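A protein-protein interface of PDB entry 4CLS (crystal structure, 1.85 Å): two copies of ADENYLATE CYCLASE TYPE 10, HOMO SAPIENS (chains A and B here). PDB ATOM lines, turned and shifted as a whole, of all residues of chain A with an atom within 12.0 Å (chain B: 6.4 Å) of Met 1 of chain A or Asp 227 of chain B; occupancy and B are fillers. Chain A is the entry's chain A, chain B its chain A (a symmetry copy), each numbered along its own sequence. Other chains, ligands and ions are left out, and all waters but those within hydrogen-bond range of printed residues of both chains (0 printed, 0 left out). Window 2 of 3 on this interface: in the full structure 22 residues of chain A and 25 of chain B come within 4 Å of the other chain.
OH of Tyr 240 of chain B sits at hydrogen-bond distance from N of Asn 2 of chain A, 3.0 Å away.
O of Ile 88 of chain B is in hydrogen-bond range of OH of Tyr 240 of chain B, 2.6 Å away. OD1 of Asn 225 of chain B is in hydrogen-bond range of N of Asp 227 of chain B (3.1 Å). O of Asp 227 of chain B lies within hydrogen-bond range of OG1 of Thr 231 of chain B, at 3.0 Å.
Among the printed residues, pairs that only touch across the chains: Met 1 of chain A with Ile 88 of chain B, Met 1 of chain A with Phe 89 of chain B, Met 1 of chain A with Phe 226 of chain B, Met 1 of chain A with Asp 227 of chain B, Met 1 of chain A with Phe 230 of chain B, Met 1 of chain A with Tyr 240 of chain B, Asn 2 of chain A with Ile 88 of chain B and Pro 4 of chain A with Ile 88 of chain B.
Met 1 of chain A touches just these residues of chain B: Ile 88 (3.7 Å), Phe 89 (3.5 Å), Phe 226 (3.7 Å), Asp 227 (3.9 Å), Phe 230 (3.3 Å) and Tyr 240 (3.6 Å). Printed residues of chain B within 4 Å of Asn 2 of chain A: Ile 88 and Tyr 240. Thr 3 of chain A touches none of the printed residues of chain B. Lys 85 of chain B touches none of the printed residues of chain A. Of chain A, only Met 1 (3.7 Å), Asn 2 (3.5 Å) and Pro 4 (3.7 Å) come within 4 Å of Ile 88 of chain B. Printed residues of chain A within 4 Å of Phe 89 of chain B: Met 1 (3.5 Å). No residue of chain A comes within 4 Å of Asn 225 of chain B. Of chain A, only Met 1 comes within 4 Å of Asp 227 of chain B. No residue of chain A comes within 4 Å of Glu 228 of chain B. No residue of chain A comes within 4 Å of Thr 231 of chain B. Of the printed residues of chain A, Tyr 240 of chain B touches Met 1 (3.6 Å) and Asn 2 (3.0 Å). The nearest residue of chain B that does not touch Met 1 of chain A is Thr 231 of chain B (4.9 Å). The nearest residue of chain A that does not touch Asp 227 of chain B is Asn 2 of chain A (7.8 Å).
Of the 16 printed residues of chain B, 6 touch a printed residue of chain A. Printed residues of chain A that touch a printed residue of chain B: Met 1, Asn 2 and Pro 4. Hydrophobic or aromatic side chains of chain A that line the printed part of chain B: Met 1 and Pro 4. Among the printed residues, no Asp or Glu carboxylate lies within 4 Å of a Lys or Arg side-chain nitrogen of the other chain.
No position is printed for both chains. Of the 9 pairs that touch across the chains among the printed residues, none has its exchanged pair printed and touching as well.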
ATOM      1  N   MET A   1     -20.939  -7.598  -5.558  1.00  0.00           N
ATOM      2  CA  MET A   1     -21.891  -6.571  -6.107  1.00  0.00           C
ATOM      3  C   MET A   1     -22.480  -6.987  -7.416  1.00  0.00           C
ATOM      4  O   MET A   1     -21.787  -7.447  -8.311  1.00  0.00           O
ATOM      5  CB  MET A   1     -21.220  -5.215  -6.305  1.00  0.00           C
ATOM      6  CG  MET A   1     -21.329  -4.318  -5.097  1.00  0.00           C
ATOM      7  SD  MET A   1     -20.640  -2.665  -5.304  1.00  0.00           S
ATOM      8  CE  MET A   1     -18.924  -3.135  -5.610  1.00  0.00           C
ATOM      9  N   ASN A   2     -23.764  -6.706  -7.606  1.00  0.00           N
ATOM     10  CA  ASN A   2     -24.409  -7.011  -8.830  1.00  0.00           C
ATOM     11  C   ASN A   2     -23.974  -6.091  -9.952  1.00  0.00           C
ATOM     12  O   ASN A   2     -23.546  -4.959  -9.716  1.00  0.00           O
ATOM     13  CB  ASN A   2     -25.938  -6.896  -8.670  1.00  0.00           C
ATOM     14  CG  ASN A   2     -26.501  -7.875  -7.655  1.00  0.00           C
ATOM     15  OD1 ASN A   2     -25.887  -8.926  -7.296  1.00  0.00           O
ATOM     16  ND2 ASN A   2     -27.634  -7.510  -7.108  1.00  0.00           N
ATOM     17  N   THR A   3     -24.147  -6.575 -11.176  1.00  0.00           N
ATOM     18  CA  THR A   3     -23.916  -5.788 -12.361  1.00  0.00           C
ATOM     19  C   THR A   3     -25.179  -5.870 -13.194  1.00  0.00           C
ATOM     20  O   THR A   3     -25.236  -6.569 -14.207  1.00  0.00           O
ATOM     21  CB  THR A   3     -22.687  -6.288 -13.133  1.00  0.00           C
ATOM     22  OG1 THR A   3     -22.844  -7.668 -13.408  1.00  0.00           O
ATOM     23  CG2 THR A   3     -21.467  -6.172 -12.299  1.00  0.00           C
ATOM     24  N   PRO A   4     -26.214  -5.139 -12.784  1.00  0.00           N
ATOM     25  CA  PRO A   4     -27.509  -5.228 -13.490  1.00  0.00           C
ATOM     26  C   PRO A   4     -27.483  -4.762 -14.926  1.00  0.00           C
ATOM     27  O   PRO A   4     -26.653  -3.963 -15.290  1.00  0.00           O
ATOM     28  CB  PRO A   4     -28.465  -4.359 -12.648  1.00  0.00           C
ATOM     29  CG  PRO A   4     -27.621  -3.634 -11.662  1.00  0.00           C
ATOM     30  CD  PRO A   4     -26.259  -4.255 -11.614  1.00  0.00           C
ATOM     31  N   LYS A   5     -28.384  -5.305 -15.739  1.00  0.00           N
ATOM     32  CA  LYS A   5     -28.486  -4.903 -17.131  1.00  0.00           C
ATOM     33  C   LYS A   5     -28.838  -3.412 -17.228  1.00  0.00           C
ATOM     34  O   LYS A   5     -29.703  -2.925 -16.494  1.00  0.00           O
ATOM     35  CB  LYS A   5     -29.557  -5.729 -17.860  1.00  0.00           C
ATOM     36  CG  LYS A   5     -29.587  -5.459 -19.362  1.00  0.00           C
ATOM     37  CD  LYS A   5     -30.488  -6.418 -20.125  1.00  0.00           C
ATOM     38  CE  LYS A   5     -30.364  -6.200 -21.629  1.00  0.00           C
ATOM     39  NZ  LYS A   5     -31.137  -7.233 -22.376  1.00  0.00           N
ATOM     40  N   LYS B  85     -26.018   3.565  -8.365  1.00  0.00           N
ATOM     41  CA  LYS B  85     -24.943   3.277  -7.431  1.00  0.00           C
ATOM     42  C   LYS B  85     -25.394   2.952  -6.030  1.00  0.00           C
ATOM     43  O   LYS B  85     -24.864   2.015  -5.432  1.00  0.00           O
ATOM     44  CB  LYS B  85     -23.977   4.423  -7.283  1.00  0.00           C
ATOM     45  CG  LYS B  85     -23.174   4.630  -8.484  1.00  0.00           C
ATOM     46  CD  LYS B  85     -21.944   3.805  -8.367  1.00  0.00           C
ATOM     47  CE  LYS B  85     -21.095   4.013  -9.610  1.00  0.00           C
ATOM     48  NZ  LYS B  85     -20.142   2.878  -9.710  1.00  0.00           N
ATOM     49  N   ILE B  88     -27.013  -0.608  -6.110  1.00  0.00           N
ATOM     50  CA  ILE B  88     -26.027  -1.684  -6.295  1.00  0.00           C
ATOM     51  C   ILE B  88     -25.209  -1.940  -5.029  1.00  0.00           C
ATOM     52  O   ILE B  88     -24.817  -3.066  -4.745  1.00  0.00           O
ATOM     53  CB  ILE B  88     -25.175  -1.341  -7.546  1.00  0.00           C
ATOM     54  CG1 ILE B  88     -26.025  -1.571  -8.798  1.00  0.00           C
ATOM     55  CG2 ILE B  88     -23.897  -2.139  -7.613  1.00  0.00           C
ATOM     56  CD1 ILE B  88     -25.440  -1.016 -10.085  1.00  0.00           C
ATOM     57  N   PHE B  89     -25.020  -0.897  -4.258  1.00  0.00           N
ATOM     58  CA  PHE B  89     -24.277  -0.940  -3.000  1.00  0.00           C
ATOM     59  C   PHE B  89     -25.222  -1.320  -1.847  1.00  0.00           C
ATOM     60  O   PHE B  89     -24.809  -1.310  -0.707  1.00  0.00           O
ATOM     61  CB  PHE B  89     -23.565   0.407  -2.710  1.00  0.00           C
ATOM     62  CG  PHE B  89     -22.196   0.540  -3.369  1.00  0.00           C
ATOM     63  CD1 PHE B  89     -22.077   0.759  -4.737  1.00  0.00           C
ATOM     64  CD2 PHE B  89     -21.029   0.397  -2.606  1.00  0.00           C
ATOM     65  CE1 PHE B  89     -20.811   0.837  -5.345  1.00  0.00           C
ATOM     66  CE2 PHE B  89     -19.776   0.451  -3.216  1.00  0.00           C
ATOM     67  CZ  PHE B  89     -19.667   0.730  -4.566  1.00  0.00           C
ATOM     68  N   LYS B 121     -17.535   3.904   0.556  1.00  0.00           N
ATOM     69  CA  LYS B 121     -17.140   3.532  -0.792  1.00  0.00           C
ATOM     70  C   LYS B 121     -18.125   3.950  -1.881  1.00  0.00           C
ATOM     71  O   LYS B 121     -17.729   4.414  -2.980  1.00  0.00           O
ATOM     72  CB  LYS B 121     -16.944   2.004  -0.884  1.00  0.00           C
ATOM     73  CG  LYS B 121     -16.356   1.498  -2.168  1.00  0.00           C
ATOM     74  CD  LYS B 121     -15.065   2.230  -2.423  1.00  0.00           C
ATOM     75  CE  LYS B 121     -14.587   2.150  -3.871  1.00  0.00           C
ATOM     76  NZ  LYS B 121     -14.034   0.785  -4.064  1.00  0.00           N
ATOM     77  N   GLU B 125     -17.543   6.535  -4.938  1.00  0.00           N
ATOM     78  CA  GLU B 125     -17.834   6.245  -6.332  1.00  0.00           C
ATOM     79  C   GLU B 125     -18.871   7.196  -6.940  1.00  0.00           C
ATOM     80  O   GLU B 125     -18.802   7.433  -8.104  1.00  0.00           O
ATOM     81  CB  GLU B 125     -18.305   4.861  -6.519  1.00  0.00           C
ATOM     82  CG  GLU B 125     -17.213   3.913  -6.216  1.00  0.00           C
ATOM     83  CD  GLU B 125     -17.488   2.567  -6.717  1.00  0.00           C
ATOM     84  OE1 GLU B 125     -18.414   2.396  -7.485  1.00  0.00           O
ATOM     85  OE2 GLU B 125     -16.730   1.678  -6.333  1.00  0.00           O
ATOM     86  N   PHE B 224      -7.150  -6.813   2.032  1.00  0.00           N
ATOM     87  CA  PHE B 224      -8.556  -6.434   1.866  1.00  0.00           C
ATOM     88  C   PHE B 224      -9.019  -6.530   0.443  1.00  0.00           C
ATOM     89  O   PHE B 224      -8.367  -6.040  -0.442  1.00  0.00           O
ATOM     90  CB  PHE B 224      -8.755  -5.015   2.283  1.00  0.00           C
ATOM     91  CG  PHE B 224     -10.206  -4.550   2.295  1.00  0.00           C
ATOM     92  CD1 PHE B 224     -11.046  -4.907   3.334  1.00  0.00           C
ATOM     93  CD2 PHE B 224     -10.680  -3.659   1.323  1.00  0.00           C
ATOM     94  CE1 PHE B 224     -12.332  -4.430   3.387  1.00  0.00           C
ATOM     95  CE2 PHE B 224     -11.965  -3.194   1.367  1.00  0.00           C
ATOM     96  CZ  PHE B 224     -12.785  -3.553   2.426  1.00  0.00           C
ATOM     97  N   ASN B 225     -10.186  -7.119   0.255  1.00  0.00           N
ATOM     98  CA  ASN B 225     -10.792  -7.289  -1.049  1.00  0.00           C
ATOM     99  C   ASN B 225     -12.224  -6.769  -0.962  1.00  0.00           C
ATOM    100  O   ASN B 225     -13.036  -7.406  -0.354  1.00  0.00           O
ATOM    101  CB  ASN B 225     -10.810  -8.757  -1.441  1.00  0.00           C
ATOM    102  CG  ASN B 225     -11.419  -8.970  -2.826  1.00  0.00           C
ATOM    103  OD1 ASN B 225     -12.621  -8.790  -3.057  1.00  0.00           O
ATOM    104  ND2 ASN B 225     -10.569  -9.298  -3.767  1.00  0.00           N
ATOM    105  N   PHE B 226     -12.499  -5.612  -1.559  1.00  0.00           N
ATOM    106  CA  PHE B 226     -13.785  -4.982  -1.409  1.00  0.00           C
ATOM    107  C   PHE B 226     -14.948  -5.881  -1.829  1.00  0.00           C
ATOM    108  O   PHE B 226     -15.960  -5.926  -1.123  1.00  0.00           O
ATOM    109  CB  PHE B 226     -13.906  -3.584  -2.066  1.00  0.00           C
ATOM    110  CG  PHE B 226     -15.199  -2.945  -1.743  1.00  0.00           C
ATOM    111  CD1 PHE B 226     -15.391  -2.347  -0.491  1.00  0.00           C
ATOM    112  CD2 PHE B 226     -16.321  -3.137  -2.576  1.00  0.00           C
ATOM    113  CE1 PHE B 226     -16.625  -1.867  -0.110  1.00  0.00           C
ATOM    114  CE2 PHE B 226     -17.543  -2.612  -2.218  1.00  0.00           C
ATOM    115  CZ  PHE B 226     -17.709  -1.975  -0.984  1.00  0.00           C
ATOM    116  N   ASP B 227     -14.798  -6.623  -2.924  1.00  0.00           N
ATOM    117  CA  ASP B 227     -15.870  -7.518  -3.402  1.00  0.00           C
ATOM    118  C   ASP B 227     -16.214  -8.656  -2.435  1.00  0.00           C
ATOM    119  O   ASP B 227     -17.391  -8.895  -2.198  1.00  0.00           O
ATOM    120  CB  ASP B 227     -15.559  -8.050  -4.802  1.00  0.00           C
ATOM    121  CG  ASP B 227     -15.494  -6.923  -5.829  1.00  0.00           C
ATOM    122  OD1 ASP B 227     -16.204  -5.912  -5.669  1.00  0.00           O
ATOM    123  OD2 ASP B 227     -14.702  -7.011  -6.785  1.00  0.00           O
ATOM    124  N   GLU B 228     -15.209  -9.293  -1.836  1.00  0.00           N
ATOM    125  CA  GLU B 228     -15.453 -10.264  -0.773  1.00  0.00           C
ATOM    126  C   GLU B 228     -16.043  -9.662   0.465  1.00  0.00           C
ATOM    127  O   GLU B 228     -16.928 -10.254   1.053  1.00  0.00           O
ATOM    128  CB  GLU B 228     -14.145 -10.956  -0.342  1.00  0.00           C
ATOM    129  CG  GLU B 228     -13.727 -11.998  -1.332  1.00  0.00           C
ATOM    130  CD  GLU B 228     -12.318 -12.485  -1.117  1.00  0.00           C
ATOM    131  OE1 GLU B 228     -11.744 -12.284  -0.010  1.00  0.00           O
ATOM    132  OE2 GLU B 228     -11.814 -13.066  -2.087  1.00  0.00           O
ATOM    133  N   PHE B 229     -15.537  -8.497   0.893  1.00  0.00           N
ATOM    134  CA  PHE B 229     -16.121  -7.782   2.024  1.00  0.00           C
ATOM    135  C   PHE B 229     -17.605  -7.436   1.783  1.00  0.00           C
ATOM    136  O   PHE B 229     -18.478  -7.605   2.676  1.00  0.00           O
ATOM    137  CB  PHE B 229     -15.350  -6.500   2.213  1.00  0.00           C
ATOM    138  CG  PHE B 229     -15.863  -5.640   3.296  1.00  0.00           C
ATOM    139  CD1 PHE B 229     -15.639  -5.967   4.609  1.00  0.00           C
ATOM    140  CD2 PHE B 229     -16.521  -4.447   3.006  1.00  0.00           C
ATOM    141  CE1 PHE B 229     -16.071  -5.143   5.647  1.00  0.00           C
ATOM    142  CE2 PHE B 229     -16.976  -3.626   4.029  1.00  0.00           C
ATOM    143  CZ  PHE B 229     -16.769  -3.980   5.350  1.00  0.00           C
ATOM    144  N   PHE B 230     -17.878  -6.940   0.598  1.00  0.00           N
ATOM    145  CA  PHE B 230     -19.259  -6.555   0.227  1.00  0.00           C
ATOM    146  C   PHE B 230     -20.130  -7.790   0.269  1.00  0.00           C
ATOM    147  O   PHE B 230     -21.220  -7.767   0.880  1.00  0.00           O
ATOM    148  CB  PHE B 230     -19.314  -5.872  -1.125  1.00  0.00           C
ATOM    149  CG  PHE B 230     -20.691  -5.401  -1.491  1.00  0.00           C
ATOM    150  CD1 PHE B 230     -21.221  -4.191  -1.004  1.00  0.00           C
ATOM    151  CD2 PHE B 230     -21.505  -6.218  -2.283  1.00  0.00           C
ATOM    152  CE1 PHE B 230     -22.511  -3.813  -1.324  1.00  0.00           C
ATOM    153  CE2 PHE B 230     -22.791  -5.865  -2.577  1.00  0.00           C
ATOM    154  CZ  PHE B 230     -23.312  -4.664  -2.090  1.00  0.00           C
ATOM    155  N   THR B 231     -19.623  -8.915  -0.252  1.00  0.00           N
ATOM    156  CA  THR B 231     -20.399 -10.133  -0.181  1.00  0.00           C
ATOM    157  C   THR B 231     -20.762 -10.498   1.273  1.00  0.00           C
ATOM    158  O   THR B 231     -21.928 -10.846   1.565  1.00  0.00           O
ATOM    159  CB  THR B 231     -19.698 -11.270  -0.883  1.00  0.00           C
ATOM    160  OG1 THR B 231     -19.621 -10.946  -2.247  1.00  0.00           O
ATOM    161  CG2 THR B 231     -20.471 -12.572  -0.711  1.00  0.00           C
ATOM    162  N   LYS B 232     -19.789 -10.422   2.169  1.00  0.00           N
ATOM    163  CA  LYS B 232     -20.086 -10.679   3.560  1.00  0.00           C
ATOM    164  C   LYS B 232     -21.157  -9.759   4.044  1.00  0.00           C
ATOM    165  O   LYS B 232     -22.078 -10.215   4.665  1.00  0.00           O
ATOM    166  CB  LYS B 232     -18.837 -10.583   4.458  1.00  0.00           C
ATOM    167  CG  LYS B 232     -17.882 -11.718   4.229  1.00  0.00           C
ATOM    168  CD  LYS B 232     -16.518 -11.584   4.984  1.00  0.00           C
ATOM    169  CE  LYS B 232     -16.643 -11.463   6.512  1.00  0.00           C
ATOM    170  NZ  LYS B 232     -16.694 -10.042   7.028  1.00  0.00           N
ATOM    171  N   THR B 234     -23.617  -8.424   2.405  1.00  0.00           N
ATOM    172  CA  THR B 234     -24.979  -8.760   1.838  1.00  0.00           C
ATOM    173  C   THR B 234     -25.763  -9.748   2.686  1.00  0.00           C
ATOM    174  O   THR B 234     -27.016  -9.787   2.646  1.00  0.00           O
ATOM    175  CB  THR B 234     -24.941  -9.282   0.375  1.00  0.00           C
ATOM    176  OG1 THR B 234     -24.230 -10.487   0.313  1.00  0.00           O
ATOM    177  CG2 THR B 234     -24.278  -8.336  -0.520  1.00  0.00           C
ATOM    178  N   TYR B 240     -31.408  -7.499  -0.950  1.00  0.00           N
ATOM    179  CA  TYR B 240     -30.439  -7.422  -2.021  1.00  0.00           C
ATOM    180  C   TYR B 240     -30.708  -8.419  -3.139  1.00  0.00           C
ATOM    181  O   TYR B 240     -30.809  -9.633  -2.883  1.00  0.00           O
ATOM    182  CB  TYR B 240     -28.998  -7.580  -1.448  1.00  0.00           C
ATOM    183  CG  TYR B 240     -27.977  -7.081  -2.457  1.00  0.00           C
ATOM    184  CD1 TYR B 240     -27.903  -5.712  -2.740  1.00  0.00           C
ATOM    185  CD2 TYR B 240     -27.081  -7.932  -3.105  1.00  0.00           C
ATOM    186  CE1 TYR B 240     -26.974  -5.242  -3.638  1.00  0.00           C
ATOM    187  CE2 TYR B 240     -26.137  -7.470  -4.017  1.00  0.00           C
ATOM    188  CZ  TYR B 240     -26.100  -6.117  -4.296  1.00  0.00           C
ATOM    189  OH  TYR B 240     -25.181  -5.595  -5.189  1.00  0.00           O
